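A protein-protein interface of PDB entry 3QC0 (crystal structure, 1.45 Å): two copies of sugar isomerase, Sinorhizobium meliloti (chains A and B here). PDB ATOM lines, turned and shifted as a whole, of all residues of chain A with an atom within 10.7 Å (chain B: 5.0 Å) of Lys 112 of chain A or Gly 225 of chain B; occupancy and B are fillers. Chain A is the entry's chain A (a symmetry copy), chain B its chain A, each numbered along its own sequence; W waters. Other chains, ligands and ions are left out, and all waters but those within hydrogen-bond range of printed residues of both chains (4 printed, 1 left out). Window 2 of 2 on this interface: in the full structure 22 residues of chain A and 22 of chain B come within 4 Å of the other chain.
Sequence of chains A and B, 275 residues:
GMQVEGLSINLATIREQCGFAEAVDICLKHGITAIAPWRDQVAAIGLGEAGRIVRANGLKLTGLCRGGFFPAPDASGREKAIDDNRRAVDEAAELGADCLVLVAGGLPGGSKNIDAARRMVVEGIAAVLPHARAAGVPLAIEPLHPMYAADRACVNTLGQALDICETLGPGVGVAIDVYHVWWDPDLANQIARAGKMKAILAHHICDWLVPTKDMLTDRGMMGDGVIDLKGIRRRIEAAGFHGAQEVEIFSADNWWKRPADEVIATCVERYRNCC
Among the printed residues, pairs that only touch across the chains: Leu 107 of chain A with Val 226 of chain B (3.6 Å), Lys 112 of chain A with Val 226 of chain B (3.4 Å), Lys 112 of chain A with Ile 227 of chain B (3.5 Å), Lys 112 of chain A with Asp 228 of chain B (3.8 Å), Ala 150 of chain A with Trp 208 of chain B (3.7 Å) and Ala 150 of chain A with Val 226 of chain B (3.8 Å).
Printed residues of chain B within 4 Å of Leu 107 of chain A: Val 226 (3.6 Å).
Lys 112 of chain A touches just these residues of chain B: Gly 225 (2.9 Å), Val 226 (3.4 Å), Ile 227 (3.5 Å) and Asp 228 (3.8 Å).
Asp 115 of chain A touches none of the printed residues of chain B.
Cys 154 of chain A touches none of the printed residues of chain B.
No residue of chain A comes within 4 Å of Asp 207 of chain B.
No residue of chain A comes within 4 Å of Leu 209 of chain B.
No residue of chain A comes within 4 Å of Gly 223 of chain B.
Asp 224 of chain B touches none of the printed residues of chain A.
Printed residues of chain A within 4 Å of Gly 225 of chain B: Lys 112.
Printed residues of chain A within 4 Å of Ile 227 of chain B: Lys 112.
Of chain A, only Lys 112 comes within 4 Å of Asp 228 of chain B.
The nearest printed residue of chain A that does not touch Trp 208 of chain B is Asp 151 of chain A (5.5 Å).
Water W1 lies within hydrogen-bond range of O of Gly 223 of chain B (2.7 Å) and NZ of Lys 112 of chain A (2.9 Å).
Water W2 bridges the backbone carbonyl oxygen (O) of Lys 112 of chain A (2.7 Å) and the backbone carbonyl oxygen (O) of Val 226 of chain B (2.8 Å).
Water W4 lies within hydrogen-bond range of OD1 of Asp 151 of chain A (2.9 Å), N of Ala 150 of chain A (3.0 Å) and NE1 of Trp 208 of chain B (3.2 Å).
Water W3 lies within hydrogen-bond range of the indole nitrogen of Trp 208 of chain B (2.9 Å), the backbone carbonyl oxygen of Leu 209 of chain B (3.0 Å) and the side-chain carboxylate of Asp 151 of chain A (3.2 Å).
No position is printed for both chains.
Of the 7 pairs that touch across the chains among the printed residues, none has its exchanged pair printed and touching as well.
The backbone NH of Ile 227 of chain B sits at hydrogen-bond distance from the side-chain carboxylate of Asp 207 of chain B, 2.9 Å away.
The backbone NH (N) of Val 226 of chain B lies within hydrogen-bond range of the side-chain carboxylate (OD1) of Asp 207 of chain B (3.1 Å).
The side-chain carboxylate (OD2) of Asp 207 of chain B lies within hydrogen-bond range of the backbone NH (N) of Gly 225 of chain B (2.9 Å).
N of Leu 107 of chain A lies within hydrogen-bond range of O of Ala 150 of chain A.
The backbone carbonyl oxygen (O) of Trp 208 of chain B sits at hydrogen-bond distance from the backbone NH (N) of Val 226 of chain B, 3.0 Å away.
Hydrophobic or aromatic side chains of chain A that line the printed part of chain B: Leu 107 and Ala 150.
Among the printed residues, no Asp or Glu carboxylate lies within 4 Å of a Lys or Arg side-chain nitrogen of the other chain.
NZ of Lys 112 of chain A is in hydrogen-bond range of O of Gly 225 of chain B, 2.9 Å away.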
ATOM      1  N   PRO A  71     -13.619 -10.301   7.978  1.00  0.00           N
ATOM      2  CA  PRO A  71     -14.676  -9.314   7.671  1.00  0.00           C
ATOM      3  C   PRO A  71     -14.346  -7.924   8.179  1.00  0.00           C
ATOM      4  O   PRO A  71     -13.734  -7.775   9.254  1.00  0.00           O
ATOM      5  CB  PRO A  71     -15.926  -9.907   8.352  1.00  0.00           C
ATOM      6  CG  PRO A  71     -15.633 -11.375   8.509  1.00  0.00           C
ATOM      7  CD  PRO A  71     -14.135 -11.421   8.769  1.00  0.00           C
ATOM      8  N   PRO A  73     -15.918  -3.539   7.462  1.00  0.00           N
ATOM      9  CA  PRO A  73     -16.975  -2.771   6.828  1.00  0.00           C
ATOM     10  C   PRO A  73     -16.629  -2.167   5.482  1.00  0.00           C
ATOM     11  O   PRO A  73     -17.535  -1.689   4.796  1.00  0.00           O
ATOM     12  CB  PRO A  73     -17.242  -1.633   7.822  1.00  0.00           C
ATOM     13  CG  PRO A  73     -16.485  -1.900   9.006  1.00  0.00           C
ATOM     14  CD  PRO A  73     -15.453  -2.942   8.713  1.00  0.00           C
ATOM     15  N   GLY A 106     -15.341 -12.208  13.254  1.00  0.00           N
ATOM     16  CA  GLY A 106     -16.781 -12.041  13.450  1.00  0.00           C
ATOM     17  C   GLY A 106     -17.406 -11.055  12.461  1.00  0.00           C
ATOM     18  O   GLY A 106     -16.842 -10.721  11.404  1.00  0.00           O
ATOM     19  N   LEU A 107     -18.586 -10.582  12.812  1.00  0.00           N
ATOM     20  CA  LEU A 107     -19.287  -9.597  12.016  1.00  0.00           C
ATOM     21  C   LEU A 107     -18.459  -8.314  11.914  1.00  0.00           C
ATOM     22  O   LEU A 107     -17.848  -7.897  12.908  1.00  0.00           O
ATOM     23  CB  LEU A 107     -20.649  -9.279  12.666  1.00  0.00           C
ATOM     24  CG  LEU A 107     -21.671 -10.395  12.524  1.00  0.00           C
ATOM     25  CD1 LEU A 107     -22.718 -10.236  13.668  1.00  0.00           C
ATOM     26  CD2 LEU A 107     -22.364 -10.364  11.166  1.00  0.00           C
ATOM     27  N   PRO A 108     -18.509  -7.644  10.754  1.00  0.00           N
ATOM     28  CA  PRO A 108     -17.996  -6.292  10.662  1.00  0.00           C
ATOM     29  C   PRO A 108     -18.724  -5.403  11.635  1.00  0.00           C
ATOM     30  O   PRO A 108     -19.937  -5.626  11.903  1.00  0.00           O
ATOM     31  CB  PRO A 108     -18.326  -5.875   9.222  1.00  0.00           C
ATOM     32  CG  PRO A 108     -18.570  -7.070   8.502  1.00  0.00           C
ATOM     33  CD  PRO A 108     -19.024  -8.139   9.474  1.00  0.00           C
ATOM     34  N   GLY A 109     -18.056  -4.415  12.207  1.00  0.00           N
ATOM     35  CA  GLY A 109     -18.750  -3.575  13.188  1.00  0.00           C
ATOM     36  C   GLY A 109     -20.059  -2.979  12.682  1.00  0.00           C
ATOM     37  O   GLY A 109     -20.117  -2.466  11.560  1.00  0.00           O
ATOM     38  N   GLY A 110     -21.084  -3.079  13.516  1.00  0.00           N
ATOM     39  CA  GLY A 110     -22.450  -2.623  13.234  1.00  0.00           C
ATOM     40  C   GLY A 110     -23.345  -3.578  12.442  1.00  0.00           C
ATOM     41  O   GLY A 110     -24.577  -3.472  12.462  1.00  0.00           O
ATOM     42  N   SER A 111     -22.745  -4.517  11.738  1.00  0.00           N
ATOM     43  CA  SER A 111     -23.501  -5.323  10.826  1.00  0.00           C
ATOM     44  C   SER A 111     -24.203  -6.476  11.519  1.00  0.00           C
ATOM     45  O   SER A 111     -23.718  -7.018  12.529  1.00  0.00           O
ATOM     46  CB  SER A 111     -22.563  -5.893   9.749  1.00  0.00           C
ATOM     47  OG  SER A 111     -23.285  -6.697   8.798  1.00  0.00           O
ATOM     48  N   LYS A 112     -25.357  -6.848  10.959  1.00  0.00           N
ATOM     49  CA  LYS A 112     -26.101  -8.039  11.333  1.00  0.00           C
ATOM     50  C   LYS A 112     -26.052  -9.083  10.235  1.00  0.00           C
ATOM     51  O   LYS A 112     -26.685 -10.140  10.330  1.00  0.00           O
ATOM     52  CB  LYS A 112     -27.585  -7.682  11.569  1.00  0.00           C
ATOM     53  CG  LYS A 112     -27.761  -6.537  12.564  1.00  0.00           C
ATOM     54  CD  LYS A 112     -29.257  -6.300  12.817  1.00  0.00           C
ATOM     55  CE  LYS A 112     -29.519  -5.021  13.615  1.00  0.00           C
ATOM     56  NZ  LYS A 112     -28.939  -5.043  14.967  1.00  0.00           N
ATOM     57  N   ASN A 113     -25.288  -8.799   9.182  1.00  0.00           N
ATOM     58  CA  ASN A 113     -25.349  -9.603   7.974  1.00  0.00           C
ATOM     59  C   ASN A 113     -24.339 -10.750   8.084  1.00  0.00           C
ATOM     60  O   ASN A 113     -23.235 -10.703   7.522  1.00  0.00           O
ATOM     61  CB  ASN A 113     -25.099  -8.742   6.740  1.00  0.00           C
ATOM     62  CG  ASN A 113     -25.518  -9.430   5.446  1.00  0.00           C
ATOM     63  OD1 ASN A 113     -25.606 -10.666   5.397  1.00  0.00           O
ATOM     64  ND2 ASN A 113     -25.781  -8.625   4.397  1.00  0.00           N
ATOM     65  N   ILE A 114     -24.733 -11.804   8.782  1.00  0.00           N
ATOM     66  CA  ILE A 114     -23.841 -12.932   9.046  1.00  0.00           C
ATOM     67  C   ILE A 114     -23.488 -13.675   7.759  1.00  0.00           C
ATOM     68  O   ILE A 114     -22.339 -14.111   7.584  1.00  0.00           O
ATOM     69  CB  ILE A 114     -24.403 -13.858  10.142  1.00  0.00           C
ATOM     70  CG1 ILE A 114     -23.367 -14.808  10.694  1.00  0.00           C
ATOM     71  CG2 ILE A 114     -25.656 -14.650   9.627  1.00  0.00           C
ATOM     72  CD1 ILE A 114     -22.238 -14.164  11.492  1.00  0.00           C
ATOM     73  N   ASP A 115     -24.428 -13.770   6.822  1.00  0.00           N
ATOM     74  CA  ASP A 115     -24.087 -14.407   5.564  1.00  0.00           C
ATOM     75  C   ASP A 115     -23.026 -13.621   4.786  1.00  0.00           C
ATOM     76  O   ASP A 115     -22.117 -14.223   4.172  1.00  0.00           O
ATOM     77  CB  ASP A 115     -25.322 -14.613   4.671  1.00  0.00           C
ATOM     78  CG  ASP A 115     -26.320 -15.612   5.219  1.00  0.00           C
ATOM     79  OD1 ASP A 115     -26.082 -16.266   6.242  1.00  0.00           O
ATOM     80  OD2 ASP A 115     -27.399 -15.741   4.542  1.00  0.00           O
ATOM     81  N   ALA A 116     -23.124 -12.296   4.779  1.00  0.00           N
ATOM     82  CA  ALA A 116     -22.136 -11.463   4.113  1.00  0.00           C
ATOM     83  C   ALA A 116     -20.794 -11.592   4.785  1.00  0.00           C
ATOM     84  O   ALA A 116     -19.742 -11.628   4.097  1.00  0.00           O
ATOM     85  CB  ALA A 116     -22.580  -9.978   4.084  1.00  0.00           C
ATOM     86  N   ALA A 117     -20.778 -11.615   6.113  1.00  0.00           N
ATOM     87  CA  ALA A 117     -19.500 -11.810   6.839  1.00  0.00           C
ATOM     88  C   ALA A 117     -18.851 -13.117   6.374  1.00  0.00           C
ATOM     89  O   ALA A 117     -17.660 -13.213   6.158  1.00  0.00           O
ATOM     90  CB  ALA A 117     -19.730 -11.815   8.358  1.00  0.00           C
ATOM     91  N   ARG A 118     -19.642 -14.157   6.250  1.00  0.00           N
ATOM     92  CA  ARG A 118     -19.121 -15.448   5.824  1.00  0.00           C
ATOM     93  C   ARG A 118     -18.612 -15.406   4.384  1.00  0.00           C
ATOM     94  O   ARG A 118     -17.566 -15.995   4.102  1.00  0.00           O
ATOM     95  CB  ARG A 118     -20.191 -16.518   6.040  1.00  0.00           C
ATOM     96  CG  ARG A 118     -20.347 -16.802   7.528  1.00  0.00           C
ATOM     97  CD  ARG A 118     -21.625 -17.539   7.894  1.00  0.00           C
ATOM     98  NE  ARG A 118     -21.531 -17.924   9.285  1.00  0.00           N
ATOM     99  CZ  ARG A 118     -22.539 -18.196  10.098  1.00  0.00           C
ATOM    100  NH1 ARG A 118     -23.760 -18.272   9.624  1.00  0.00           N
ATOM    101  NH2 ARG A 118     -22.300 -18.478  11.368  1.00  0.00           N
ATOM    102  N   ARG A 119     -19.319 -14.686   3.503  1.00  0.00           N
ATOM    103  CA  ARG A 119     -18.794 -14.484   2.145  1.00  0.00           C
ATOM    104  C   ARG A 119     -17.434 -13.773   2.189  1.00  0.00           C
ATOM    105  O   ARG A 119     -16.525 -14.095   1.409  1.00  0.00           O
ATOM    106  CB  ARG A 119     -19.753 -13.701   1.263  1.00  0.00           C
ATOM    107  CG  ARG A 119     -20.990 -14.488   0.904  1.00  0.00           C
ATOM    108  CD  ARG A 119     -21.802 -13.818  -0.197  1.00  0.00           C
ATOM    109  NE  ARG A 119     -22.278 -12.482   0.170  1.00  0.00           N
ATOM    110  CZ  ARG A 119     -23.438 -12.229   0.784  1.00  0.00           C
ATOM    111  NH1 ARG A 119     -24.247 -13.203   1.151  1.00  0.00           N
ATOM    112  NH2 ARG A 119     -23.775 -10.975   1.038  1.00  0.00           N
ATOM    113  N   MET A 120     -17.278 -12.796   3.058  1.00  0.00           N
ATOM    114  CA  MET A 120     -15.974 -12.073   3.203  1.00  0.00           C
ATOM    115  C   MET A 120     -14.888 -12.992   3.670  1.00  0.00           C
ATOM    116  O   MET A 120     -13.748 -12.851   3.256  1.00  0.00           O
ATOM    117  CB  MET A 120     -16.096 -10.908   4.156  1.00  0.00           C
ATOM    118  CG  MET A 120     -17.028  -9.797   3.723  1.00  0.00           C
ATOM    119  SD  MET A 120     -17.295  -8.484   5.082  1.00  0.00           S
ATOM    120  CE  MET A 120     -18.544  -7.340   4.180  1.00  0.00           C
ATOM    121  N   ALA A 149     -19.357 -16.718  17.348  1.00  0.00           N
ATOM    122  CA  ALA A 149     -19.798 -16.345  16.009  1.00  0.00           C
ATOM    123  C   ALA A 149     -19.820 -14.860  15.737  1.00  0.00           C
ATOM    124  O   ALA A 149     -19.541 -14.430  14.628  1.00  0.00           O
ATOM    125  CB  ALA A 149     -21.184 -16.983  15.672  1.00  0.00           C
ATOM    126  N   ALA A 150     -20.288 -14.070  16.712  1.00  0.00           N
ATOM    127  CA  ALA A 150     -20.537 -12.653  16.445  1.00  0.00           C
ATOM    128  C   ALA A 150     -19.285 -11.816  16.381  1.00  0.00           C
ATOM    129  O   ALA A 150     -19.253 -10.837  15.662  1.00  0.00           O
ATOM    130  CB  ALA A 150     -21.494 -12.040  17.497  1.00  0.00           C
ATOM    131  N   ASP A 151     -18.315 -12.165  17.212  1.00  0.00           N
ATOM    132  CA  ASP A 151     -17.206 -11.259  17.472  1.00  0.00           C
ATOM    133  C   ASP A 151     -15.817 -11.839  17.356  1.00  0.00           C
ATOM    134  O   ASP A 151     -14.862 -11.073  17.535  1.00  0.00           O
ATOM    135  CB  ASP A 151     -17.425 -10.548  18.802  1.00  0.00           C
ATOM    136  CG  ASP A 151     -17.529 -11.466  19.969  1.00  0.00           C
ATOM    137  OD1 ASP A 151     -17.564 -12.705  19.826  1.00  0.00           O
ATOM    138  OD2 ASP A 151     -17.553 -10.889  21.107  1.00  0.00           O
ATOM    139  N   CYS A 154     -16.900 -16.387  12.461  1.00  0.00           N
ATOM    140  CA  CYS A 154     -18.194 -16.791  11.933  1.00  0.00           C
ATOM    141  C   CYS A 154     -18.120 -18.052  11.051  1.00  0.00           C
ATOM    142  O   CYS A 154     -19.070 -18.356  10.366  1.00  0.00           O
ATOM    143  CB  CYS A 154     -18.827 -15.621  11.189  1.00  0.00           C
ATOM    144  SG  CYS A 154     -17.907 -15.116   9.678  1.00  0.00           S
ATOM    145  N   ASP B 207     -31.883 -10.848  21.717  1.00  0.00           N
ATOM    146  CA  ASP B 207     -30.742 -10.541  20.890  1.00  0.00           C
ATOM    147  C   ASP B 207     -29.447 -11.089  21.477  1.00  0.00           C
ATOM    148  O   ASP B 207     -29.378 -11.400  22.678  1.00  0.00           O
ATOM    149  CB  ASP B 207     -30.618  -9.013  20.662  1.00  0.00           C
ATOM    150  CG  ASP B 207     -30.218  -8.652  19.224  1.00  0.00           C
ATOM    151  OD1 ASP B 207     -29.529  -9.483  18.546  1.00  0.00           O
ATOM    152  OD2 ASP B 207     -30.556  -7.518  18.764  1.00  0.00           O
ATOM    153  N   TRP B 208     -28.455 -11.211  20.598  1.00  0.00           N
ATOM    154  CA  TRP B 208     -27.114 -11.638  20.947  1.00  0.00           C
ATOM    155  C   TRP B 208     -26.207 -10.427  21.029  1.00  0.00           C
ATOM    156  O   TRP B 208     -25.966  -9.767  20.025  1.00  0.00           O
ATOM    157  CB  TRP B 208     -26.589 -12.663  19.908  1.00  0.00           C
ATOM    158  CG  TRP B 208     -25.237 -13.197  20.318  1.00  0.00           C
ATOM    159  CD1 TRP B 208     -24.011 -12.608  20.087  1.00  0.00           C
ATOM    160  CD2 TRP B 208     -24.959 -14.382  21.072  1.00  0.00           C
ATOM    161  NE1 TRP B 208     -23.013 -13.382  20.609  1.00  0.00           N
ATOM    162  CE2 TRP B 208     -23.566 -14.471  21.227  1.00  0.00           C
ATOM    163  CE3 TRP B 208     -25.730 -15.404  21.560  1.00  0.00           C
ATOM    164  CZ2 TRP B 208     -22.968 -15.510  21.910  1.00  0.00           C
ATOM    165  CZ3 TRP B 208     -25.148 -16.423  22.256  1.00  0.00           C
ATOM    166  CH2 TRP B 208     -23.772 -16.492  22.400  1.00  0.00           C
ATOM    167  N   LEU B 209     -25.755 -10.119  22.241  1.00  0.00           N
ATOM    168  CA  LEU B 209     -24.955  -8.912  22.476  1.00  0.00           C
ATOM    169  C   LEU B 209     -23.494  -9.108  22.111  1.00  0.00           C
ATOM    170  O   LEU B 209     -22.965 -10.202  22.227  1.00  0.00           O
ATOM    171  CB  LEU B 209     -25.091  -8.478  23.938  1.00  0.00           C
ATOM    172  CG  LEU B 209     -26.508  -8.140  24.426  1.00  0.00           C
ATOM    173  CD1 LEU B 209     -26.415  -7.844  25.941  1.00  0.00           C
ATOM    174  CD2 LEU B 209     -27.111  -7.007  23.566  1.00  0.00           C
ATOM    175  N   MET B 221     -31.966  -7.216  24.762  1.00  0.00           N
ATOM    176  CA  MET B 221     -33.181  -6.694  24.217  1.00  0.00           C
ATOM    177  C   MET B 221     -33.031  -6.629  22.695  1.00  0.00           C
ATOM    178  O   MET B 221     -31.972  -6.256  22.167  1.00  0.00           O
ATOM    179  CB  MET B 221     -33.405  -5.290  24.789  1.00  0.00           C
ATOM    180  CG  MET B 221     -34.620  -4.552  24.291  1.00  0.00           C
ATOM    181  SD  MET B 221     -36.332  -5.356  24.639  1.00  0.00           S
ATOM    182  CE  MET B 221     -36.228  -5.027  26.594  1.00  0.00           C
ATOM    183  N   GLY B 223     -32.638  -5.591  19.137  1.00  0.00           N
ATOM    184  CA  GLY B 223     -32.037  -4.384  18.581  1.00  0.00           C
ATOM    185  C   GLY B 223     -30.774  -3.904  19.267  1.00  0.00           C
ATOM    186  O   GLY B 223     -30.081  -3.027  18.729  1.00  0.00           O
ATOM    187  N   ASP B 224     -30.476  -4.424  20.449  1.00  0.00           N
ATOM    188  CA  ASP B 224     -29.261  -4.057  21.155  1.00  0.00           C
ATOM    189  C   ASP B 224     -28.102  -4.939  20.714  1.00  0.00           C
ATOM    190  O   ASP B 224     -26.933  -4.642  21.032  1.00  0.00           O
ATOM    191  CB  ASP B 224     -29.429  -4.176  22.679  1.00  0.00           C
ATOM    192  CG  ASP B 224     -30.209  -3.008  23.310  1.00  0.00           C
ATOM    193  OD1 ASP B 224     -30.522  -2.030  22.587  1.00  0.00           O
ATOM    194  OD2 ASP B 224     -30.410  -3.069  24.546  1.00  0.00           O
ATOM    195  N   GLY B 225     -28.409  -6.030  19.997  1.00  0.00           N
ATOM    196  CA  GLY B 225     -27.367  -6.970  19.551  1.00  0.00           C
ATOM    197  C   GLY B 225     -27.287  -7.074  18.040  1.00  0.00           C
ATOM    198  O   GLY B 225     -27.633  -6.144  17.322  1.00  0.00           O
ATOM    199  N   VAL B 226     -26.827  -8.239  17.561  1.00  0.00           N
ATOM    200  CA  VAL B 226     -26.426  -8.443  16.177  1.00  0.00           C
ATOM    201  C   VAL B 226     -27.284  -9.388  15.374  1.00  0.00           C
ATOM    202  O   VAL B 226     -26.968  -9.661  14.209  1.00  0.00           O
ATOM    203  CB  VAL B 226     -24.972  -8.953  16.110  1.00  0.00           C
ATOM    204  CG1 VAL B 226     -24.051  -7.946  16.762  1.00  0.00           C
ATOM    205  CG2 VAL B 226     -24.856 -10.372  16.674  1.00  0.00           C
ATOM    206  N   ILE B 227     -28.347  -9.926  15.948  1.00  0.00           N
ATOM    207  CA  ILE B 227     -29.163 -10.886  15.216  1.00  0.00           C
ATOM    208  C   ILE B 227     -30.004 -10.193  14.167  1.00  0.00           C
ATOM    209  O   ILE B 227     -30.602  -9.161  14.422  1.00  0.00           O
ATOM    210  CB  ILE B 227     -30.086 -11.709  16.158  1.00  0.00           C
ATOM    211  CG1 ILE B 227     -29.238 -12.505  17.176  1.00  0.00           C
ATOM    212  CG2 ILE B 227     -31.006 -12.634  15.344  1.00  0.00           C
ATOM    213  CD1 ILE B 227     -30.035 -13.390  18.118  1.00  0.00           C
ATOM    214  N   ASP B 228     -30.050 -10.767  12.977  1.00  0.00           N
ATOM    215  CA  ASP B 228     -30.932 -10.283  11.915  1.00  0.00           C
ATOM    216  C   ASP B 228     -32.338 -10.790  12.204  1.00  0.00           C
ATOM    217  O   ASP B 228     -32.822 -11.730  11.548  1.00  0.00           O
ATOM    218  CB  ASP B 228     -30.387 -10.784  10.585  1.00  0.00           C
ATOM    219  CG  ASP B 228     -31.220 -10.378   9.370  1.00  0.00           C
ATOM    220  OD1 ASP B 228     -32.179  -9.588   9.487  1.00  0.00           O
ATOM    221  OD2 ASP B 228     -30.900 -10.880   8.238  1.00  0.00           O
HETATM  222  O   HOH W   1     -29.931  -2.603  16.096  1.00  0.00           O
HETATM  223  O   HOH W   2     -26.282 -11.744  12.483  1.00  0.00           O
HETATM  224  O   HOH W   3     -20.648 -11.705  21.129  1.00  0.00           O
HETATM  225  O   HOH W   4     -20.044 -14.199  19.706  1.00  0.00           O
